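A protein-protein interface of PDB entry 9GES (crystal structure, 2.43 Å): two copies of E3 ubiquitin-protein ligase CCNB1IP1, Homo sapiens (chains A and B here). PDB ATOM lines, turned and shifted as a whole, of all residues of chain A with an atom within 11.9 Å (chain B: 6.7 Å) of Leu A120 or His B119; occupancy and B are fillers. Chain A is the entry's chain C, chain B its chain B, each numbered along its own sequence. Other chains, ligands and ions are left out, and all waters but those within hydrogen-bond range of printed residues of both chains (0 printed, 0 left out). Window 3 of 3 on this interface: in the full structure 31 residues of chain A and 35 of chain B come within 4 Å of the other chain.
OG1 of Thr A128 is in hydrogen-bond range of O of Glu A124 (2.8 Å).
ND1 of His B119 touches CD2 of Leu A120 (3.8 Å).
Leu A120 touches Leu B120 (CD1 to CD1, 3.7 Å).
Leu A120 touches Met B123 (CD1 to CE, 3.6 Å).
Glu A124 touches Met B123 (CG to SD, 3.5 Å).
Met B123 touches Tyr A127 (CG to CD2, 3.7 Å).
Glu B124 touches Tyr A127.
Tyr A111 touches none of the printed residues of chain B.
Lys A121 touches none of the printed residues of chain B.
Of the printed residues of chain B, Glu A124 touches Met B123.
Ala B116 touches none of the printed residues of chain A.
No residue of chain A comes within 4 Å of Gly B118.
His B119 touches one residue of chain A.
Of chain A, only Leu A120 comes within 4 Å of Leu B120.
No residue of chain A comes within 4 Å of Lys B121.
Met B123 touches just these residues of chain A: Leu A120, Glu A124 and Tyr A127.
Printed residues of chain A within 4 Å of Glu B124: Tyr A127 (3.2 Å).
The nearest residue of chain A that does not touch His B119 is Glu A124 (4.04 Å).
Hydrophobic or aromatic side chains of chain A within 4 Å of the printed part of chain B: Leu A120 and Tyr A127.
Along chain A the printed residues that touch a printed residue of chain B span positions 120 to 127.
Of the 11 printed residues of chain B, 4 touch a printed residue of chain A.
Hydrophobic or aromatic side chains of chain B within 4 Å of the printed part of chain A: His B119, Leu B120 and Met B123.
Along chain B the printed residues that touch a printed residue of chain A span positions 119 to 124.
Among the printed residues, 6 pairs touch across the chains.
Among the printed residues, no Asp or Glu carboxylate lies within 4 Å of a Lys or Arg side-chain nitrogen of the other chain.
Leu A120 touches His B119, but with the chains exchanged His A119 does not touch Leu B120 (4.7 Å).
Leu B120 touches its own counterpart, Leu A120.
Leu A120 touches Met B123, but with the chains exchanged Met A123 does not touch Leu B120 (4.3 Å).
Glu A124 touches Met B123, but with the chains exchanged Met A123 does not touch Glu B124 (5.7 Å).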
ATOM      1  N   TYR A 111      -1.656  29.899 -30.870  1.00  0.00           N
ATOM      2  CA  TYR A 111      -1.256  29.168 -29.671  1.00  0.00           C
ATOM      3  C   TYR A 111      -1.983  29.688 -28.435  1.00  0.00           C
ATOM      4  O   TYR A 111      -2.402  28.903 -27.576  1.00  0.00           O
ATOM      5  CB  TYR A 111       0.258  29.256 -29.484  1.00  0.00           C
ATOM      6  CG  TYR A 111       0.723  28.836 -28.109  1.00  0.00           C
ATOM      7  CD1 TYR A 111       0.763  27.498 -27.746  1.00  0.00           C
ATOM      8  CD2 TYR A 111       1.124  29.782 -27.174  1.00  0.00           C
ATOM      9  CE1 TYR A 111       1.185  27.111 -26.488  1.00  0.00           C
ATOM     10  CE2 TYR A 111       1.548  29.405 -25.915  1.00  0.00           C
ATOM     11  CZ  TYR A 111       1.577  28.070 -25.577  1.00  0.00           C
ATOM     12  OH  TYR A 111       2.001  27.692 -24.324  1.00  0.00           O
ATOM     13  N   ASN A 112      -2.131  31.012 -28.323  1.00  0.00           N
ATOM     14  CA  ASN A 112      -2.871  31.580 -27.200  1.00  0.00           C
ATOM     15  C   ASN A 112      -4.333  31.156 -27.230  1.00  0.00           C
ATOM     16  O   ASN A 112      -4.929  30.879 -26.182  1.00  0.00           O
ATOM     17  CB  ASN A 112      -2.757  33.104 -27.210  1.00  0.00           C
ATOM     18  CG  ASN A 112      -1.442  33.593 -26.643  1.00  0.00           C
ATOM     19  OD1 ASN A 112      -0.529  32.807 -26.390  1.00  0.00           O
ATOM     20  ND2 ASN A 112      -1.338  34.901 -26.439  1.00  0.00           N
ATOM     21  N   PHE A 113      -4.934  31.116 -28.422  1.00  0.00           N
ATOM     22  CA  PHE A 113      -6.317  30.663 -28.534  1.00  0.00           C
ATOM     23  C   PHE A 113      -6.452  29.205 -28.111  1.00  0.00           C
ATOM     24  O   PHE A 113      -7.415  28.835 -27.430  1.00  0.00           O
ATOM     25  CB  PHE A 113      -6.824  30.859 -29.964  1.00  0.00           C
ATOM     26  CG  PHE A 113      -8.308  30.668 -30.112  1.00  0.00           C
ATOM     27  CD1 PHE A 113      -9.180  31.720 -29.881  1.00  0.00           C
ATOM     28  CD2 PHE A 113      -8.833  29.440 -30.484  1.00  0.00           C
ATOM     29  CE1 PHE A 113     -10.546  31.551 -30.015  1.00  0.00           C
ATOM     30  CE2 PHE A 113     -10.197  29.265 -30.620  1.00  0.00           C
ATOM     31  CZ  PHE A 113     -11.055  30.322 -30.385  1.00  0.00           C
ATOM     32  N   SER A 114      -5.496  28.363 -28.512  1.00  0.00           N
ATOM     33  CA  SER A 114      -5.522  26.964 -28.096  1.00  0.00           C
ATOM     34  C   SER A 114      -5.367  26.834 -26.587  1.00  0.00           C
ATOM     35  O   SER A 114      -6.047  26.019 -25.953  1.00  0.00           O
ATOM     36  CB  SER A 114      -4.426  26.182 -28.820  1.00  0.00           C
ATOM     37  OG  SER A 114      -4.601  26.247 -30.225  1.00  0.00           O
ATOM     38  N   LYS A 115      -4.470  27.627 -25.994  1.00  0.00           N
ATOM     39  CA  LYS A 115      -4.312  27.611 -24.543  1.00  0.00           C
ATOM     40  C   LYS A 115      -5.585  28.079 -23.846  1.00  0.00           C
ATOM     41  O   LYS A 115      -5.985  27.512 -22.822  1.00  0.00           O
ATOM     42  CB  LYS A 115      -3.126  28.484 -24.136  1.00  0.00           C
ATOM     43  CG  LYS A 115      -2.926  28.592 -22.634  1.00  0.00           C
ATOM     44  CD  LYS A 115      -1.834  29.591 -22.301  1.00  0.00           C
ATOM     45  CE  LYS A 115      -0.522  29.206 -22.959  1.00  0.00           C
ATOM     46  NZ  LYS A 115       0.551  30.199 -22.682  1.00  0.00           N
ATOM     47  N   ALA A 116      -6.229  29.119 -24.382  1.00  0.00           N
ATOM     48  CA  ALA A 116      -7.468  29.610 -23.788  1.00  0.00           C
ATOM     49  C   ALA A 116      -8.569  28.558 -23.852  1.00  0.00           C
ATOM     50  O   ALA A 116      -9.321  28.377 -22.887  1.00  0.00           O
ATOM     51  CB  ALA A 116      -7.909  30.896 -24.486  1.00  0.00           C
ATOM     52  N   GLU A 117      -8.684  27.858 -24.985  1.00  0.00           N
ATOM     53  CA  GLU A 117      -9.692  26.809 -25.112  1.00  0.00           C
ATOM     54  C   GLU A 117      -9.443  25.677 -24.123  1.00  0.00           C
ATOM     55  O   GLU A 117     -10.385  25.152 -23.518  1.00  0.00           O
ATOM     56  CB  GLU A 117      -9.718  26.270 -26.544  1.00  0.00           C
ATOM     57  CG  GLU A 117     -10.291  27.233 -27.572  1.00  0.00           C
ATOM     58  CD  GLU A 117     -11.799  27.373 -27.474  1.00  0.00           C
ATOM     59  OE1 GLU A 117     -12.436  26.546 -26.788  1.00  0.00           O
ATOM     60  OE2 GLU A 117     -12.349  28.313 -28.088  1.00  0.00           O
ATOM     61  N   GLY A 118      -8.181  25.274 -23.960  1.00  0.00           N
ATOM     62  CA  GLY A 118      -7.867  24.239 -22.991  1.00  0.00           C
ATOM     63  C   GLY A 118      -8.152  24.672 -21.565  1.00  0.00           C
ATOM     64  O   GLY A 118      -8.682  23.898 -20.765  1.00  0.00           O
ATOM     65  N   HIS A 119      -7.802  25.916 -21.230  1.00  0.00           N
ATOM     66  CA  HIS A 119      -8.137  26.447 -19.912  1.00  0.00           C
ATOM     67  C   HIS A 119      -9.646  26.522 -19.719  1.00  0.00           C
ATOM     68  O   HIS A 119     -10.156  26.218 -18.634  1.00  0.00           O
ATOM     69  CB  HIS A 119      -7.501  27.824 -19.720  1.00  0.00           C
ATOM     70  CG  HIS A 119      -7.831  28.465 -18.406  1.00  0.00           C
ATOM     71  ND1 HIS A 119      -8.022  29.822 -18.267  1.00  0.00           N
ATOM     72  CD2 HIS A 119      -7.998  27.933 -17.172  1.00  0.00           C
ATOM     73  CE1 HIS A 119      -8.297  30.099 -17.005  1.00  0.00           C
ATOM     74  NE2 HIS A 119      -8.288  28.970 -16.319  1.00  0.00           N
ATOM     75  N   LEU A 120     -10.377  26.924 -20.762  1.00  0.00           N
ATOM     76  CA  LEU A 120     -11.830  27.024 -20.662  1.00  0.00           C
ATOM     77  C   LEU A 120     -12.458  25.665 -20.372  1.00  0.00           C
ATOM     78  O   LEU A 120     -13.322  25.545 -19.497  1.00  0.00           O
ATOM     79  CB  LEU A 120     -12.401  27.620 -21.949  1.00  0.00           C
ATOM     80  CG  LEU A 120     -13.916  27.819 -22.021  1.00  0.00           C
ATOM     81  CD1 LEU A 120     -14.382  28.832 -20.986  1.00  0.00           C
ATOM     82  CD2 LEU A 120     -14.335  28.246 -23.418  1.00  0.00           C
ATOM     83  N   LYS A 121     -12.022  24.625 -21.088  1.00  0.00           N
ATOM     84  CA  LYS A 121     -12.574  23.291 -20.865  1.00  0.00           C
ATOM     85  C   LYS A 121     -12.194  22.755 -19.490  1.00  0.00           C
ATOM     86  O   LYS A 121     -12.985  22.047 -18.855  1.00  0.00           O
ATOM     87  CB  LYS A 121     -12.109  22.337 -21.964  1.00  0.00           C
ATOM     88  CG  LYS A 121     -12.676  22.665 -23.331  1.00  0.00           C
ATOM     89  CD  LYS A 121     -12.152  21.720 -24.397  1.00  0.00           C
ATOM     90  CE  LYS A 121     -12.717  22.073 -25.763  1.00  0.00           C
ATOM     91  NZ  LYS A 121     -12.156  21.221 -26.845  1.00  0.00           N
ATOM     92  N   GLN A 122     -10.984  23.066 -19.019  1.00  0.00           N
ATOM     93  CA  GLN A 122     -10.597  22.670 -17.668  1.00  0.00           C
ATOM     94  C   GLN A 122     -11.467  23.361 -16.625  1.00  0.00           C
ATOM     95  O   GLN A 122     -11.837  22.753 -15.614  1.00  0.00           O
ATOM     96  CB  GLN A 122      -9.118  22.977 -17.427  1.00  0.00           C
ATOM     97  CG  GLN A 122      -8.154  22.081 -18.195  1.00  0.00           C
ATOM     98  CD  GLN A 122      -8.194  20.635 -17.735  1.00  0.00           C
ATOM     99  OE1 GLN A 122      -8.561  20.342 -16.596  1.00  0.00           O
ATOM    100  NE2 GLN A 122      -7.818  19.721 -18.623  1.00  0.00           N
ATOM    101  N   MET A 123     -11.798  24.635 -16.849  1.00  0.00           N
ATOM    102  CA  MET A 123     -12.679  25.342 -15.924  1.00  0.00           C
ATOM    103  C   MET A 123     -14.082  24.747 -15.929  1.00  0.00           C
ATOM    104  O   MET A 123     -14.740  24.689 -14.882  1.00  0.00           O
ATOM    105  CB  MET A 123     -12.718  26.832 -16.269  1.00  0.00           C
ATOM    106  CG  MET A 123     -11.397  27.541 -16.037  1.00  0.00           C
ATOM    107  SD  MET A 123     -10.715  27.186 -14.408  1.00  0.00           S
ATOM    108  CE  MET A 123     -11.990  27.873 -13.355  1.00  0.00           C
ATOM    109  N   GLU A 124     -14.562  24.309 -17.098  1.00  0.00           N
ATOM    110  CA  GLU A 124     -15.863  23.649 -17.165  1.00  0.00           C
ATOM    111  C   GLU A 124     -15.874  22.369 -16.340  1.00  0.00           C
ATOM    112  O   GLU A 124     -16.784  22.151 -15.532  1.00  0.00           O
ATOM    113  CB  GLU A 124     -16.227  23.331 -18.616  1.00  0.00           C
ATOM    114  CG  GLU A 124     -16.287  24.523 -19.551  1.00  0.00           C
ATOM    115  CD  GLU A 124     -16.618  24.128 -20.981  1.00  0.00           C
ATOM    116  OE1 GLU A 124     -17.028  22.969 -21.203  1.00  0.00           O
ATOM    117  OE2 GLU A 124     -16.462  24.977 -21.886  1.00  0.00           O
ATOM    118  N   LYS A 125     -14.814  21.540 -16.431  1.00  0.00           N
ATOM    119  CA  LYS A 125     -14.698  20.346 -15.567  1.00  0.00           C
ATOM    120  C   LYS A 125     -14.628  20.726 -14.093  1.00  0.00           C
ATOM    121  O   LYS A 125     -15.287  20.103 -13.254  1.00  0.00           O
ATOM    122  CB  LYS A 125     -13.468  19.520 -15.965  1.00  0.00           C
ATOM    123  CG  LYS A 125     -13.243  18.274 -15.127  1.00  0.00           C
ATOM    124  CD  LYS A 125     -11.918  17.615 -15.483  1.00  0.00           C
ATOM    125  CE  LYS A 125     -11.663  16.392 -14.618  1.00  0.00           C
ATOM    126  NZ  LYS A 125     -10.323  15.793 -14.867  1.00  0.00           N
ATOM    127  N   ILE A 126     -13.834  21.746 -13.760  1.00  0.00           N
ATOM    128  CA  ILE A 126     -13.668  22.134 -12.361  1.00  0.00           C
ATOM    129  C   ILE A 126     -14.992  22.621 -11.782  1.00  0.00           C
ATOM    130  O   ILE A 126     -15.390  22.226 -10.679  1.00  0.00           O
ATOM    131  CB  ILE A 126     -12.565  23.201 -12.224  1.00  0.00           C
ATOM    132  CG1 ILE A 126     -11.194  22.588 -12.519  1.00  0.00           C
ATOM    133  CG2 ILE A 126     -12.587  23.816 -10.833  1.00  0.00           C
ATOM    134  CD1 ILE A 126     -10.063  23.593 -12.521  1.00  0.00           C
ATOM    135  N   TYR A 127     -15.697  23.478 -12.523  1.00  0.00           N
ATOM    136  CA  TYR A 127     -16.956  24.018 -12.019  1.00  0.00           C
ATOM    137  C   TYR A 127     -18.010  22.929 -11.858  1.00  0.00           C
ATOM    138  O   TYR A 127     -18.719  22.892 -10.846  1.00  0.00           O
ATOM    139  CB  TYR A 127     -17.460  25.130 -12.939  1.00  0.00           C
ATOM    140  CG  TYR A 127     -16.689  26.423 -12.793  1.00  0.00           C
ATOM    141  CD1 TYR A 127     -15.880  26.648 -11.686  1.00  0.00           C
ATOM    142  CD2 TYR A 127     -16.772  27.418 -13.758  1.00  0.00           C
ATOM    143  CE1 TYR A 127     -15.173  27.827 -11.545  1.00  0.00           C
ATOM    144  CE2 TYR A 127     -16.068  28.601 -13.626  1.00  0.00           C
ATOM    145  CZ  TYR A 127     -15.272  28.800 -12.518  1.00  0.00           C
ATOM    146  OH  TYR A 127     -14.570  29.974 -12.381  1.00  0.00           O
ATOM    147  N   THR A 128     -18.122  22.028 -12.839  1.00  0.00           N
ATOM    148  CA  THR A 128     -19.107  20.956 -12.745  1.00  0.00           C
ATOM    149  C   THR A 128     -18.809  20.026 -11.575  1.00  0.00           C
ATOM    150  O   THR A 128     -19.727  19.594 -10.868  1.00  0.00           O
ATOM    151  CB  THR A 128     -19.158  20.168 -14.054  1.00  0.00           C
ATOM    152  OG1 THR A 128     -17.832  19.763 -14.418  1.00  0.00           O
ATOM    153  CG2 THR A 128     -19.757  21.017 -15.168  1.00  0.00           C
ATOM    154  N   GLN A 129     -17.531  19.699 -11.359  1.00  0.00           N
ATOM    155  CA  GLN A 129     -17.167  18.858 -10.222  1.00  0.00           C
ATOM    156  C   GLN A 129     -17.481  19.548  -8.901  1.00  0.00           C
ATOM    157  O   GLN A 129     -17.977  18.913  -7.962  1.00  0.00           O
ATOM    158  CB  GLN A 129     -15.685  18.483 -10.291  1.00  0.00           C
ATOM    159  CG  GLN A 129     -15.349  17.460 -11.362  1.00  0.00           C
ATOM    160  CD  GLN A 129     -13.914  16.975 -11.275  1.00  0.00           C
ATOM    161  OE1 GLN A 129     -13.103  17.528 -10.533  1.00  0.00           O
ATOM    162  NE2 GLN A 129     -13.596  15.931 -12.031  1.00  0.00           N
ATOM    163  N   GLN A 130     -17.197  20.849  -8.807  1.00  0.00           N
ATOM    164  CA  GLN A 130     -17.519  21.584  -7.589  1.00  0.00           C
ATOM    165  C   GLN A 130     -19.025  21.710  -7.393  1.00  0.00           C
ATOM    166  O   GLN A 130     -19.500  21.736  -6.252  1.00  0.00           O
ATOM    167  CB  GLN A 130     -16.848  22.956  -7.623  1.00  0.00           C
ATOM    168  CG  GLN A 130     -15.334  22.874  -7.504  1.00  0.00           C
ATOM    169  CD  GLN A 130     -14.643  24.174  -7.859  1.00  0.00           C
ATOM    170  OE1 GLN A 130     -15.256  25.081  -8.415  1.00  0.00           O
ATOM    171  NE2 GLN A 130     -13.356  24.269  -7.542  1.00  0.00           N
ATOM    172  N   SER B 114     -12.288  37.221 -27.986  1.00  0.00           N
ATOM    173  CA  SER B 114     -13.208  37.995 -27.157  1.00  0.00           C
ATOM    174  C   SER B 114     -14.456  37.187 -26.820  1.00  0.00           C
ATOM    175  O   SER B 114     -14.961  37.251 -25.692  1.00  0.00           O
ATOM    176  CB  SER B 114     -13.584  39.297 -27.865  1.00  0.00           C
ATOM    177  OG  SER B 114     -12.432  40.070 -28.151  1.00  0.00           O
ATOM    178  N   LYS B 115     -14.972  36.427 -27.789  1.00  0.00           N
ATOM    179  CA  LYS B 115     -16.134  35.580 -27.538  1.00  0.00           C
ATOM    180  C   LYS B 115     -15.828  34.516 -26.490  1.00  0.00           C
ATOM    181  O   LYS B 115     -16.670  34.217 -25.634  1.00  0.00           O
ATOM    182  CB  LYS B 115     -16.595  34.932 -28.844  1.00  0.00           C
ATOM    183  CG  LYS B 115     -17.755  33.964 -28.685  1.00  0.00           C
ATOM    184  CD  LYS B 115     -18.060  33.264 -30.000  1.00  0.00           C
ATOM    185  CE  LYS B 115     -18.349  34.270 -31.101  1.00  0.00           C
ATOM    186  NZ  LYS B 115     -18.598  33.610 -32.412  1.00  0.00           N
ATOM    187  N   ALA B 116     -14.631  33.926 -26.548  1.00  0.00           N
ATOM    188  CA  ALA B 116     -14.239  32.941 -25.545  1.00  0.00           C
ATOM    189  C   ALA B 116     -14.134  33.573 -24.162  1.00  0.00           C
ATOM    190  O   ALA B 116     -14.547  32.970 -23.163  1.00  0.00           O
ATOM    191  CB  ALA B 116     -12.915  32.288 -25.941  1.00  0.00           C
ATOM    192  N   GLU B 117     -13.578  34.785 -24.083  1.00  0.00           N
ATOM    193  CA  GLU B 117     -13.498  35.483 -22.803  1.00  0.00           C
ATOM    194  C   GLU B 117     -14.887  35.769 -22.246  1.00  0.00           C
ATOM    195  O   GLU B 117     -15.124  35.621 -21.041  1.00  0.00           O
ATOM    196  CB  GLU B 117     -12.706  36.781 -22.960  1.00  0.00           C
ATOM    197  CG  GLU B 117     -11.226  36.588 -23.264  1.00  0.00           C
ATOM    198  CD  GLU B 117     -10.422  36.172 -22.046  1.00  0.00           C
ATOM    199  OE1 GLU B 117     -10.956  36.246 -20.920  1.00  0.00           O
ATOM    200  OE2 GLU B 117      -9.250  35.772 -22.217  1.00  0.00           O
ATOM    201  N   GLY B 118     -15.817  36.181 -23.110  1.00  0.00           N
ATOM    202  CA  GLY B 118     -17.177  36.427 -22.658  1.00  0.00           C
ATOM    203  C   GLY B 118     -17.858  35.176 -22.138  1.00  0.00           C
ATOM    204  O   GLY B 118     -18.562  35.216 -21.126  1.00  0.00           O
ATOM    205  N   HIS B 119     -17.662  34.047 -22.827  1.00  0.00           N
ATOM    206  CA  HIS B 119     -18.251  32.791 -22.370  1.00  0.00           C
ATOM    207  C   HIS B 119     -17.684  32.373 -21.020  1.00  0.00           C
ATOM    208  O   HIS B 119     -18.417  31.875 -20.157  1.00  0.00           O
ATOM    209  CB  HIS B 119     -18.020  31.692 -23.406  1.00  0.00           C
ATOM    210  CG  HIS B 119     -18.599  30.367 -23.016  1.00  0.00           C
ATOM    211  ND1 HIS B 119     -17.998  29.169 -23.334  1.00  0.00           N
ATOM    212  CD2 HIS B 119     -19.726  30.054 -22.335  1.00  0.00           C
ATOM    213  CE1 HIS B 119     -18.729  28.174 -22.864  1.00  0.00           C
ATOM    214  NE2 HIS B 119     -19.784  28.683 -22.254  1.00  0.00           N
ATOM    215  N   LEU B 120     -16.376  32.555 -20.825  1.00  0.00           N
ATOM    216  CA  LEU B 120     -15.765  32.214 -19.545  1.00  0.00           C
ATOM    217  C   LEU B 120     -16.341  33.058 -18.414  1.00  0.00           C
ATOM    218  O   LEU B 120     -16.632  32.538 -17.331  1.00  0.00           O
ATOM    219  CB  LEU B 120     -14.248  32.389 -19.627  1.00  0.00           C
ATOM    220  CG  LEU B 120     -13.467  32.136 -18.336  1.00  0.00           C
ATOM    221  CD1 LEU B 120     -13.630  30.693 -17.884  1.00  0.00           C
ATOM    222  CD2 LEU B 120     -11.998  32.485 -18.517  1.00  0.00           C
ATOM    223  N   LYS B 121     -16.516  34.362 -18.649  1.00  0.00           N
ATOM    224  CA  LYS B 121     -17.066  35.236 -17.617  1.00  0.00           C
ATOM    225  C   LYS B 121     -18.509  34.870 -17.286  1.00  0.00           C
ATOM    226  O   LYS B 121     -18.910  34.897 -16.116  1.00  0.00           O
ATOM    227  CB  LYS B 121     -16.964  36.697 -18.059  1.00  0.00           C
ATOM    228  CG  LYS B 121     -15.546  37.249 -18.018  1.00  0.00           C
ATOM    229  CD  LYS B 121     -15.492  38.700 -18.472  1.00  0.00           C
ATOM    230  CE  LYS B 121     -15.805  38.835 -19.954  1.00  0.00           C
ATOM    231  NZ  LYS B 121     -15.630  40.235 -20.438  1.00  0.00           N
ATOM    232  N   GLN B 122     -19.308  34.538 -18.303  1.00  0.00           N
ATOM    233  CA  GLN B 122     -20.669  34.072 -18.053  1.00  0.00           C
ATOM    234  C   GLN B 122     -20.666  32.756 -17.287  1.00  0.00           C
ATOM    235  O   GLN B 122     -21.535  32.518 -16.439  1.00  0.00           O
ATOM    236  CB  GLN B 122     -21.426  33.921 -19.374  1.00  0.00           C
ATOM    237  CG  GLN B 122     -21.687  35.233 -20.094  1.00  0.00           C
ATOM    238  CD  GLN B 122     -22.692  36.104 -19.366  1.00  0.00           C
ATOM    239  OE1 GLN B 122     -23.505  35.611 -18.585  1.00  0.00           O
ATOM    240  NE2 GLN B 122     -22.640  37.407 -19.620  1.00  0.00           N
ATOM    241  N   MET B 123     -19.700  31.884 -17.582  1.00  0.00           N
ATOM    242  CA  MET B 123     -19.600  30.604 -16.889  1.00  0.00           C
ATOM    243  C   MET B 123     -19.296  30.795 -15.407  1.00  0.00           C
ATOM    244  O   MET B 123     -19.915  30.158 -14.547  1.00  0.00           O
ATOM    245  CB  MET B 123     -18.526  29.749 -17.556  1.00  0.00           C
ATOM    246  CG  MET B 123     -18.326  28.383 -16.941  1.00  0.00           C
ATOM    247  SD  MET B 123     -17.032  27.513 -17.834  1.00  0.00           S
ATOM    248  CE  MET B 123     -17.551  27.831 -19.521  1.00  0.00           C
ATOM    249  N   GLU B 124     -18.335  31.668 -15.089  1.00  0.00           N
ATOM    250  CA  GLU B 124     -18.060  31.990 -13.692  1.00  0.00           C
ATOM    251  C   GLU B 124     -19.265  32.658 -13.041  1.00  0.00           C
ATOM    252  O   GLU B 124     -19.548  32.435 -11.858  1.00  0.00           O
ATOM    253  CB  GLU B 124     -16.829  32.895 -13.591  1.00  0.00           C
ATOM    254  CG  GLU B 124     -15.600  32.372 -14.317  1.00  0.00           C
ATOM    255  CD  GLU B 124     -14.466  33.382 -14.339  1.00  0.00           C
ATOM    256  OE1 GLU B 124     -14.572  34.415 -13.643  1.00  0.00           O
ATOM    257  OE2 GLU B 124     -13.471  33.142 -15.056  1.00  0.00           O
